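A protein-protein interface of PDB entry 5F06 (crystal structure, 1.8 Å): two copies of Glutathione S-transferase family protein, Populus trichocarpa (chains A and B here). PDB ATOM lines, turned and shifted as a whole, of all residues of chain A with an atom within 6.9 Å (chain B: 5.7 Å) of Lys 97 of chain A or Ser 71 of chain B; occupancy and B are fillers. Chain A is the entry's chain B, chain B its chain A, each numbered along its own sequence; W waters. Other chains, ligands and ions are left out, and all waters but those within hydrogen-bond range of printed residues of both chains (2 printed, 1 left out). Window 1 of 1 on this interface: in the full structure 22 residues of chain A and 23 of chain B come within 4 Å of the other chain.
The side-chain amino group (NZ) of Lys 97 of chain A lies within hydrogen-bond range of the side-chain hydroxyl (OG) of Ser 71 of chain B (2.8 Å).
Hydrophobic or aromatic side chains of chain B within 4 Å of the printed part of chain A: Ala 68 and Tyr 72.
Of the printed residues of chain B, Lys 97 of chain A touches Ala 68, Ser 71 and Tyr 72.
Of the printed residues of chain A, Ser 71 of chain B touches Lys 97.
Of the printed residues of chain A, Glu 65 of chain B touches Val 98 and Glu 101.
Of the printed residues of chain A, Ala 68 of chain B touches Lys 97 (3.6 Å), Val 98 (3.6 Å) and Glu 101 (3.7 Å).
Of the printed residues of chain B, Ala 94 of chain A touches Tyr 72.
Of the printed residues of chain B, Glu 101 of chain A touches Glu 65 (3.7 Å), Arg 67 (3.5 Å) and Ala 68 (3.7 Å).
Cys 19 of chain B touches none of the printed residues of chain A.
Ala 74 of chain B touches none of the printed residues of chain A.
The nearest printed residue of chain B that does not touch Lys 97 of chain A is Glu 75 of chain B (4.7 Å).
The nearest residue of chain A that does not touch Ser 71 of chain B is Glu 101 of chain A (6.5 Å).
Among the printed residues, merely in contact across the chains: Ala 94 of chain A with Tyr 72 of chain B, Lys 97 of chain A with Ala 68 of chain B, Lys 97 of chain A with Tyr 72 of chain B, Val 98 of chain A with Glu 65 of chain B, Val 98 of chain A with Ala 68 of chain B, Glu 101 of chain A with Glu 65 of chain B, Glu 101 of chain A with Arg 67 of chain B and Glu 101 of chain A with Ala 68 of chain B.
Water W1 lies within hydrogen-bond range of the side-chain carboxylate of Glu 65 of chain B, the side-chain carboxylate of Glu 101 of chain A and the guanidinium group of Arg 67 of chain B.
Water W2 bridges OE2 of Glu 75 of chain B and NZ of Lys 97 of chain A.
The side-chain hydroxyl (OG) of Ser 66 of chain B is in hydrogen-bond range of the guanidinium group (NH1) of Arg 67 of chain B (3.5 Å).
The side-chain hydroxyl of Tyr 72 of chain B sits at hydrogen-bond distance from the side-chain amino group of Lys 76 of chain B, at 3.2 Å.
O of Lys 97 of chain A sits at hydrogen-bond distance from OG1 of Thr 100 of chain A, 2.9 Å away.
O of Arg 67 of chain B lies within hydrogen-bond range of OG1 of Thr 70 of chain B.
2 positions are printed for both chains.
Of the 9 pairs that touch across the chains among the printed residues, none has its exchanged pair printed and touching as well.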
ATOM      1  N   SER A  71      13.110  30.262 -15.499  1.00  0.00           N
ATOM      2  CA  SER A  71      13.191  29.044 -16.304  1.00  0.00           C
ATOM      3  C   SER A  71      13.573  29.372 -17.746  1.00  0.00           C
ATOM      4  O   SER A  71      14.347  28.652 -18.370  1.00  0.00           O
ATOM      5  CB  SER A  71      11.865  28.284 -16.270  1.00  0.00           C
ATOM      6  OG  SER A  71      11.913  27.155 -17.125  1.00  0.00           O
ATOM      7  N   ILE A  85      20.135  24.269 -14.359  1.00  0.00           N
ATOM      8  CA  ILE A  85      19.151  23.233 -14.678  1.00  0.00           C
ATOM      9  C   ILE A  85      19.768  21.873 -15.015  1.00  0.00           C
ATOM     10  O   ILE A  85      19.041  20.912 -15.267  1.00  0.00           O
ATOM     11  CB  ILE A  85      18.262  23.665 -15.863  1.00  0.00           C
ATOM     12  CG1 ILE A  85      19.101  23.881 -17.128  1.00  0.00           C
ATOM     13  CG2 ILE A  85      17.492  24.927 -15.505  1.00  0.00           C
ATOM     14  CD1 ILE A  85      18.276  23.932 -18.400  1.00  0.00           C
ATOM     15  N   LEU A  90      20.548  14.347 -17.530  1.00  0.00           N
ATOM     16  CA  LEU A  90      19.090  14.328 -17.615  1.00  0.00           C
ATOM     17  C   LEU A  90      18.432  13.890 -16.305  1.00  0.00           C
ATOM     18  O   LEU A  90      17.298  14.272 -16.023  1.00  0.00           O
ATOM     19  CB  LEU A  90      18.644  13.413 -18.760  1.00  0.00           C
ATOM     20  CG  LEU A  90      17.137  13.312 -19.028  1.00  0.00           C
ATOM     21  CD1 LEU A  90      16.487  14.686 -19.136  1.00  0.00           C
ATOM     22  CD2 LEU A  90      16.884  12.513 -20.300  1.00  0.00           C
ATOM     23  N   GLU A  92      19.862  14.447 -13.139  1.00  0.00           N
ATOM     24  CA  GLU A  92      20.004  15.624 -12.288  1.00  0.00           C
ATOM     25  C   GLU A  92      18.986  16.672 -12.706  1.00  0.00           C
ATOM     26  O   GLU A  92      18.365  17.311 -11.861  1.00  0.00           O
ATOM     27  CB  GLU A  92      21.421  16.201 -12.360  1.00  0.00           C
ATOM     28  CG  GLU A  92      22.491  15.314 -11.729  1.00  0.00           C
ATOM     29  CD  GLU A  92      23.877  15.937 -11.758  1.00  0.00           C
ATOM     30  OE1 GLU A  92      24.832  15.274 -11.301  1.00  0.00           O
ATOM     31  OE2 GLU A  92      24.022  17.082 -12.238  1.00  0.00           O
ATOM     32  N   ALA A  93      18.808  16.834 -14.014  1.00  0.00           N
ATOM     33  CA  ALA A  93      17.820  17.773 -14.539  1.00  0.00           C
ATOM     34  C   ALA A  93      16.416  17.449 -14.020  1.00  0.00           C
ATOM     35  O   ALA A  93      15.668  18.343 -13.625  1.00  0.00           O
ATOM     36  CB  ALA A  93      17.841  17.759 -16.061  1.00  0.00           C
ATOM     37  N   ALA A  94      16.068  16.168 -14.020  1.00  0.00           N
ATOM     38  CA  ALA A  94      14.766  15.729 -13.531  1.00  0.00           C
ATOM     39  C   ALA A  94      14.610  16.032 -12.043  1.00  0.00           C
ATOM     40  O   ALA A  94      13.549  16.467 -11.594  1.00  0.00           O
ATOM     41  CB  ALA A  94      14.579  14.248 -13.791  1.00  0.00           C
ATOM     42  N   SER A  95      15.675  15.808 -11.281  1.00  0.00           N
ATOM     43  CA  SER A  95      15.643  16.067  -9.846  1.00  0.00           C
ATOM     44  C   SER A  95      15.406  17.551  -9.561  1.00  0.00           C
ATOM     45  O   SER A  95      14.679  17.908  -8.639  1.00  0.00           O
ATOM     46  CB  SER A  95      16.946  15.602  -9.192  1.00  0.00           C
ATOM     47  OG  SER A  95      16.881  15.740  -7.783  1.00  0.00           O
ATOM     48  N   VAL A  96      16.013  18.416 -10.365  1.00  0.00           N
ATOM     49  CA  VAL A  96      15.804  19.849 -10.209  1.00  0.00           C
ATOM     50  C   VAL A  96      14.322  20.182 -10.428  1.00  0.00           C
ATOM     51  O   VAL A  96      13.751  20.965  -9.674  1.00  0.00           O
ATOM     52  CB  VAL A  96      16.698  20.662 -11.172  1.00  0.00           C
ATOM     53  CG1 VAL A  96      16.348  22.149 -11.126  1.00  0.00           C
ATOM     54  CG2 VAL A  96      18.165  20.468 -10.818  1.00  0.00           C
ATOM     55  N   LYS A  97      13.699  19.567 -11.432  1.00  0.00           N
ATOM     56  CA  LYS A  97      12.280  19.802 -11.708  1.00  0.00           C
ATOM     57  C   LYS A  97      11.407  19.425 -10.507  1.00  0.00           C
ATOM     58  O   LYS A  97      10.466  20.139 -10.165  1.00  0.00           O
ATOM     59  CB  LYS A  97      11.822  19.014 -12.934  1.00  0.00           C
ATOM     60  CG  LYS A  97      12.460  19.432 -14.248  1.00  0.00           C
ATOM     61  CD  LYS A  97      11.923  18.595 -15.402  1.00  0.00           C
ATOM     62  CE  LYS A  97      12.394  19.118 -16.746  1.00  0.00           C
ATOM     63  NZ  LYS A  97      11.804  20.441 -17.063  1.00  0.00           N
ATOM     64  N   VAL A  98      11.720  18.303  -9.877  1.00  0.00           N
ATOM     65  CA  VAL A  98      10.985  17.858  -8.697  1.00  0.00           C
ATOM     66  C   VAL A  98      10.988  18.939  -7.625  1.00  0.00           C
ATOM     67  O   VAL A  98       9.941  19.286  -7.075  1.00  0.00           O
ATOM     68  CB  VAL A  98      11.585  16.557  -8.119  1.00  0.00           C
ATOM     69  CG1 VAL A  98      10.981  16.222  -6.751  1.00  0.00           C
ATOM     70  CG2 VAL A  98      11.375  15.416  -9.085  1.00  0.00           C
ATOM     71  N   TRP A  99      12.160  19.487  -7.337  1.00  0.00           N
ATOM     72  CA  TRP A  99      12.290  20.352  -6.176  1.00  0.00           C
ATOM     73  C   TRP A  99      11.942  21.809  -6.471  1.00  0.00           C
ATOM     74  O   TRP A  99      11.644  22.561  -5.546  1.00  0.00           O
ATOM     75  CB  TRP A  99      13.694  20.215  -5.592  1.00  0.00           C
ATOM     76  CG  TRP A  99      13.830  18.879  -4.928  1.00  0.00           C
ATOM     77  CD1 TRP A  99      14.352  17.739  -5.467  1.00  0.00           C
ATOM     78  CD2 TRP A  99      13.382  18.532  -3.613  1.00  0.00           C
ATOM     79  NE1 TRP A  99      14.273  16.710  -4.563  1.00  0.00           N
ATOM     80  CE2 TRP A  99      13.685  17.171  -3.417  1.00  0.00           C
ATOM     81  CE3 TRP A  99      12.767  19.247  -2.581  1.00  0.00           C
ATOM     82  CZ2 TRP A  99      13.392  16.508  -2.223  1.00  0.00           C
ATOM     83  CZ3 TRP A  99      12.478  18.585  -1.395  1.00  0.00           C
ATOM     84  CH2 TRP A  99      12.794  17.232  -1.227  1.00  0.00           C
ATOM     85  N   THR A 100      11.930  22.204  -7.743  1.00  0.00           N
ATOM     86  CA  THR A 100      11.333  23.487  -8.093  1.00  0.00           C
ATOM     87  C   THR A 100       9.818  23.401  -7.917  1.00  0.00           C
ATOM     88  O   THR A 100       9.193  24.366  -7.500  1.00  0.00           O
ATOM     89  CB  THR A 100      11.656  23.943  -9.537  1.00  0.00           C
ATOM     90  OG1 THR A 100      11.233  22.951 -10.477  1.00  0.00           O
ATOM     91  CG2 THR A 100      13.145  24.205  -9.704  1.00  0.00           C
ATOM     92  N   GLU A 101       9.227  22.248  -8.226  1.00  0.00           N
ATOM     93  CA  GLU A 101       7.792  22.068  -8.018  1.00  0.00           C
ATOM     94  C   GLU A 101       7.474  22.019  -6.526  1.00  0.00           C
ATOM     95  O   GLU A 101       6.424  22.492  -6.087  1.00  0.00           O
ATOM     96  CB  GLU A 101       7.293  20.808  -8.722  1.00  0.00           C
ATOM     97  CG  GLU A 101       7.147  20.992 -10.224  1.00  0.00           C
ATOM     98  CD  GLU A 101       6.104  22.039 -10.571  1.00  0.00           C
ATOM     99  OE1 GLU A 101       4.993  21.972 -10.011  1.00  0.00           O
ATOM    100  OE2 GLU A 101       6.393  22.931 -11.392  1.00  0.00           O
ATOM    101  N   VAL A 102       8.392  21.465  -5.741  1.00  0.00           N
ATOM    102  CA  VAL A 102       8.217  21.449  -4.297  1.00  0.00           C
ATOM    103  C   VAL A 102       8.189  22.893  -3.783  1.00  0.00           C
ATOM    104  O   VAL A 102       7.322  23.253  -2.983  1.00  0.00           O
ATOM    105  CB  VAL A 102       9.323  20.630  -3.601  1.00  0.00           C
ATOM    106  CG1 VAL A 102       9.364  20.907  -2.108  1.00  0.00           C
ATOM    107  CG2 VAL A 102       9.096  19.145  -3.836  1.00  0.00           C
ATOM    108  N   ALA A 158      18.291  19.157  -4.762  1.00  0.00           N
ATOM    109  CA  ALA A 158      18.160  18.242  -5.900  1.00  0.00           C
ATOM    110  C   ALA A 158      19.332  17.272  -6.015  1.00  0.00           C
ATOM    111  O   ALA A 158      19.284  16.324  -6.796  1.00  0.00           O
ATOM    112  CB  ALA A 158      18.015  19.031  -7.193  1.00  0.00           C
ATOM    113  N   SER A 163      21.281  24.333  -7.620  1.00  0.00           N
ATOM    114  CA  SER A 163      20.425  24.365  -8.802  1.00  0.00           C
ATOM    115  C   SER A 163      19.330  25.407  -8.677  1.00  0.00           C
ATOM    116  O   SER A 163      19.218  26.098  -7.658  1.00  0.00           O
ATOM    117  CB  SER A 163      19.797  22.989  -9.047  1.00  0.00           C
ATOM    118  OG  SER A 163      18.808  22.694  -8.080  1.00  0.00           O
ATOM    119  N   ALA A 165      16.381  24.890  -8.156  1.00  0.00           N
ATOM    120  CA  ALA A 165      15.493  24.522  -7.056  1.00  0.00           C
ATOM    121  C   ALA A 165      15.873  25.286  -5.796  1.00  0.00           C
ATOM    122  O   ALA A 165      15.012  25.838  -5.117  1.00  0.00           O
ATOM    123  CB  ALA A 165      15.536  23.018  -6.798  1.00  0.00           C
ATOM    124  N   CYS B  19      -0.983  13.243 -19.744  1.00  0.00           N
ATOM    125  CA  CYS B  19       0.281  13.587 -20.390  1.00  0.00           C
ATOM    126  C   CYS B  19       0.901  12.359 -21.062  1.00  0.00           C
ATOM    127  O   CYS B  19       1.343  12.429 -22.211  1.00  0.00           O
ATOM    128  CB  CYS B  19       1.267  14.185 -19.382  1.00  0.00           C
ATOM    129  SG  CYS B  19       2.890  14.615 -20.099  1.00  0.00           S
ATOM    130  N   GLU B  65       5.851  14.989  -7.446  1.00  0.00           N
ATOM    131  CA  GLU B  65       5.193  16.206  -7.954  1.00  0.00           C
ATOM    132  C   GLU B  65       4.709  15.974  -9.382  1.00  0.00           C
ATOM    133  O   GLU B  65       5.497  15.756 -10.309  1.00  0.00           O
ATOM    134  CB  GLU B  65       6.099  17.446  -7.892  1.00  0.00           C
ATOM    135  CG  GLU B  65       6.327  17.951  -6.488  1.00  0.00           C
ATOM    136  CD  GLU B  65       5.043  18.456  -5.847  1.00  0.00           C
ATOM    137  OE1 GLU B  65       4.231  19.093  -6.557  1.00  0.00           O
ATOM    138  OE2 GLU B  65       4.843  18.205  -4.639  1.00  0.00           O
ATOM    139  N   SER B  66       3.389  16.019  -9.540  1.00  0.00           N
ATOM    140  CA  SER B  66       2.754  15.650 -10.795  1.00  0.00           C
ATOM    141  C   SER B  66       3.300  16.454 -11.964  1.00  0.00           C
ATOM    142  O   SER B  66       3.507  15.910 -13.042  1.00  0.00           O
ATOM    143  CB  SER B  66       1.236  15.838 -10.704  1.00  0.00           C
ATOM    144  OG  SER B  66       0.904  17.179 -10.387  1.00  0.00           O
ATOM    145  N   ARG B  67       3.541  17.741 -11.746  1.00  0.00           N
ATOM    146  CA  ARG B  67       3.952  18.626 -12.832  1.00  0.00           C
ATOM    147  C   ARG B  67       5.456  18.528 -13.117  1.00  0.00           C
ATOM    148  O   ARG B  67       5.920  18.931 -14.187  1.00  0.00           O
ATOM    149  CB  ARG B  67       3.561  20.067 -12.510  1.00  0.00           C
ATOM    150  CG  ARG B  67       2.056  20.273 -12.276  1.00  0.00           C
ATOM    151  CD  ARG B  67       1.791  21.617 -11.613  1.00  0.00           C
ATOM    152  NE  ARG B  67       0.381  21.848 -11.297  1.00  0.00           N
ATOM    153  CZ  ARG B  67      -0.260  21.304 -10.266  1.00  0.00           C
ATOM    154  NH1 ARG B  67       0.369  20.473  -9.441  1.00  0.00           N
ATOM    155  NH2 ARG B  67      -1.540  21.586 -10.063  1.00  0.00           N
ATOM    156  N   ALA B  68       6.221  18.005 -12.164  1.00  0.00           N
ATOM    157  CA  ALA B  68       7.621  17.675 -12.432  1.00  0.00           C
ATOM    158  C   ALA B  68       7.665  16.446 -13.334  1.00  0.00           C
ATOM    159  O   ALA B  68       8.490  16.344 -14.249  1.00  0.00           O
ATOM    160  CB  ALA B  68       8.385  17.425 -11.141  1.00  0.00           C
ATOM    161  N   ILE B  69       6.755  15.516 -13.079  1.00  0.00           N
ATOM    162  CA  ILE B  69       6.703  14.278 -13.843  1.00  0.00           C
ATOM    163  C   ILE B  69       6.254  14.558 -15.275  1.00  0.00           C
ATOM    164  O   ILE B  69       6.827  14.036 -16.225  1.00  0.00           O
ATOM    165  CB  ILE B  69       5.759  13.253 -13.183  1.00  0.00           C
ATOM    166  CG1 ILE B  69       6.314  12.831 -11.820  1.00  0.00           C
ATOM    167  CG2 ILE B  69       5.599  12.033 -14.071  1.00  0.00           C
ATOM    168  CD1 ILE B  69       5.329  12.060 -10.945  1.00  0.00           C
ATOM    169  N   THR B  70       5.232  15.387 -15.438  1.00  0.00           N
ATOM    170  CA  THR B  70       4.762  15.731 -16.778  1.00  0.00           C
ATOM    171  C   THR B  70       5.835  16.490 -17.557  1.00  0.00           C
ATOM    172  O   THR B  70       6.049  16.230 -18.740  1.00  0.00           O
ATOM    173  CB  THR B  70       3.483  16.580 -16.742  1.00  0.00           C
ATOM    174  OG1 THR B  70       3.698  17.756 -15.949  1.00  0.00           O
ATOM    175  CG2 THR B  70       2.311  15.775 -16.174  1.00  0.00           C
ATOM    176  N   SER B  71       6.499  17.427 -16.888  1.00  0.00           N
ATOM    177  CA  SER B  71       7.549  18.224 -17.509  1.00  0.00           C
ATOM    178  C   SER B  71       8.703  17.327 -17.964  1.00  0.00           C
ATOM    179  O   SER B  71       9.234  17.480 -19.067  1.00  0.00           O
ATOM    180  CB  SER B  71       8.051  19.298 -16.533  1.00  0.00           C
ATOM    181  OG  SER B  71       9.025  20.137 -17.130  1.00  0.00           O
ATOM    182  N   TYR B  72       9.080  16.387 -17.107  1.00  0.00           N
ATOM    183  CA  TYR B  72      10.107  15.409 -17.445  1.00  0.00           C
ATOM    184  C   TYR B  72       9.725  14.612 -18.688  1.00  0.00           C
ATOM    185  O   TYR B  72      10.493  14.527 -19.649  1.00  0.00           O
ATOM    186  CB  TYR B  72      10.337  14.463 -16.267  1.00  0.00           C
ATOM    187  CG  TYR B  72      11.306  13.361 -16.580  1.00  0.00           C
ATOM    188  CD1 TYR B  72      12.645  13.643 -16.817  1.00  0.00           C
ATOM    189  CD2 TYR B  72      10.892  12.038 -16.639  1.00  0.00           C
ATOM    190  CE1 TYR B  72      13.543  12.644 -17.105  1.00  0.00           C
ATOM    191  CE2 TYR B  72      11.789  11.024 -16.929  1.00  0.00           C
ATOM    192  CZ  TYR B  72      13.113  11.336 -17.160  1.00  0.00           C
ATOM    193  OH  TYR B  72      14.022  10.342 -17.447  1.00  0.00           O
ATOM    194  N   ILE B  73       8.531  14.031 -18.658  1.00  0.00           N
ATOM    195  CA  ILE B  73       8.026  13.230 -19.767  1.00  0.00           C
ATOM    196  C   ILE B  73       7.950  14.057 -21.051  1.00  0.00           C
ATOM    197  O   ILE B  73       8.388  13.611 -22.115  1.00  0.00           O
ATOM    198  CB  ILE B  73       6.636  12.650 -19.423  1.00  0.00           C
ATOM    199  CG1 ILE B  73       6.771  11.608 -18.308  1.00  0.00           C
ATOM    200  CG2 ILE B  73       5.982  12.018 -20.646  1.00  0.00           C
ATOM    201  CD1 ILE B  73       5.446  11.177 -17.703  1.00  0.00           C
ATOM    202  N   ALA B  74       7.409  15.265 -20.945  1.00  0.00           N
ATOM    203  CA  ALA B  74       7.251  16.137 -22.104  1.00  0.00           C
ATOM    204  C   ALA B  74       8.598  16.508 -22.726  1.00  0.00           C
ATOM    205  O   ALA B  74       8.727  16.586 -23.947  1.00  0.00           O
ATOM    206  CB  ALA B  74       6.485  17.394 -21.715  1.00  0.00           C
ATOM    207  N   GLU B  75       9.603  16.724 -21.885  1.00  0.00           N
ATOM    208  CA  GLU B  75      10.929  17.096 -22.361  1.00  0.00           C
ATOM    209  C   GLU B  75      11.677  15.890 -22.936  1.00  0.00           C
ATOM    210  O   GLU B  75      12.308  15.988 -23.988  1.00  0.00           O
ATOM    211  CB  GLU B  75      11.738  17.735 -21.227  1.00  0.00           C
ATOM    212  CG  GLU B  75      13.208  17.982 -21.547  1.00  0.00           C
ATOM    213  CD  GLU B  75      13.400  18.927 -22.717  1.00  0.00           C
ATOM    214  OE1 GLU B  75      14.348  18.715 -23.503  1.00  0.00           O
ATOM    215  OE2 GLU B  75      12.607  19.884 -22.850  1.00  0.00           O
ATOM    216  N   LYS B  76      11.597  14.756 -22.248  1.00  0.00           N
ATOM    217  CA  LYS B  76      12.384  13.588 -22.621  1.00  0.00           C
ATOM    218  C   LYS B  76      11.929  12.984 -23.946  1.00  0.00           C
ATOM    219  O   LYS B  76      12.751  12.538 -24.746  1.00  0.00           O
ATOM    220  CB  LYS B  76      12.318  12.523 -21.524  1.00  0.00           C
ATOM    221  CG  LYS B  76      13.029  11.230 -21.903  1.00  0.00           C
ATOM    222  CD  LYS B  76      13.266  10.342 -20.703  1.00  0.00           C
ATOM    223  CE  LYS B  76      13.907   9.028 -21.106  1.00  0.00           C
ATOM    224  NZ  LYS B  76      14.488   8.332 -19.926  1.00  0.00           N
ATOM    225  N   ILE B  85       5.384  20.957 -25.132  1.00  0.00           N
ATOM    226  CA  ILE B  85       6.181  22.085 -24.641  1.00  0.00           C
ATOM    227  C   ILE B  85       6.889  22.851 -25.762  1.00  0.00           C
ATOM    228  O   ILE B  85       7.703  23.736 -25.499  1.00  0.00           O
ATOM    229  CB  ILE B  85       7.219  21.625 -23.591  1.00  0.00           C
ATOM    230  CG1 ILE B  85       8.185  20.588 -24.176  1.00  0.00           C
ATOM    231  CG2 ILE B  85       6.494  21.064 -22.363  1.00  0.00           C
ATOM    232  CD1 ILE B  85       9.377  20.293 -23.276  1.00  0.00           C
ATOM    233  N   LEU B 164       1.137  22.020 -22.576  1.00  0.00           N
ATOM    234  CA  LEU B 164       1.204  21.526 -21.205  1.00  0.00           C
ATOM    235  C   LEU B 164       0.466  22.456 -20.241  1.00  0.00           C
ATOM    236  O   LEU B 164      -0.074  22.010 -19.227  1.00  0.00           O
ATOM    237  CB  LEU B 164       2.664  21.370 -20.775  1.00  0.00           C
ATOM    238  CG  LEU B 164       2.892  20.659 -19.441  1.00  0.00           C
ATOM    239  CD1 LEU B 164       2.501  19.187 -19.530  1.00  0.00           C
ATOM    240  CD2 LEU B 164       4.346  20.814 -19.019  1.00  0.00           C
ATOM    241  N   HIS B 168      -2.460  20.880 -17.646  1.00  0.00           N
ATOM    242  CA  HIS B 168      -2.377  20.857 -16.193  1.00  0.00           C
ATOM    243  C   HIS B 168      -3.694  21.245 -15.525  1.00  0.00           C
ATOM    244  O   HIS B 168      -3.904  20.926 -14.358  1.00  0.00           O
ATOM    245  CB  HIS B 168      -1.252  21.771 -15.704  1.00  0.00           C
ATOM    246  CG  HIS B 168       0.110  21.184 -15.881  1.00  0.00           C
ATOM    247  ND1 HIS B 168       1.265  21.894 -15.642  1.00  0.00           N
ATOM    248  CD2 HIS B 168       0.501  19.946 -16.272  1.00  0.00           C
ATOM    249  CE1 HIS B 168       2.312  21.122 -15.882  1.00  0.00           C
ATOM    250  NE2 HIS B 168       1.876  19.936 -16.265  1.00  0.00           N
HETATM  251  O   HOH W   1       3.355  19.622  -9.170  1.00  0.00           O
HETATM  252  O   HOH W   2      11.817  21.086 -20.192  1.00  0.00           O
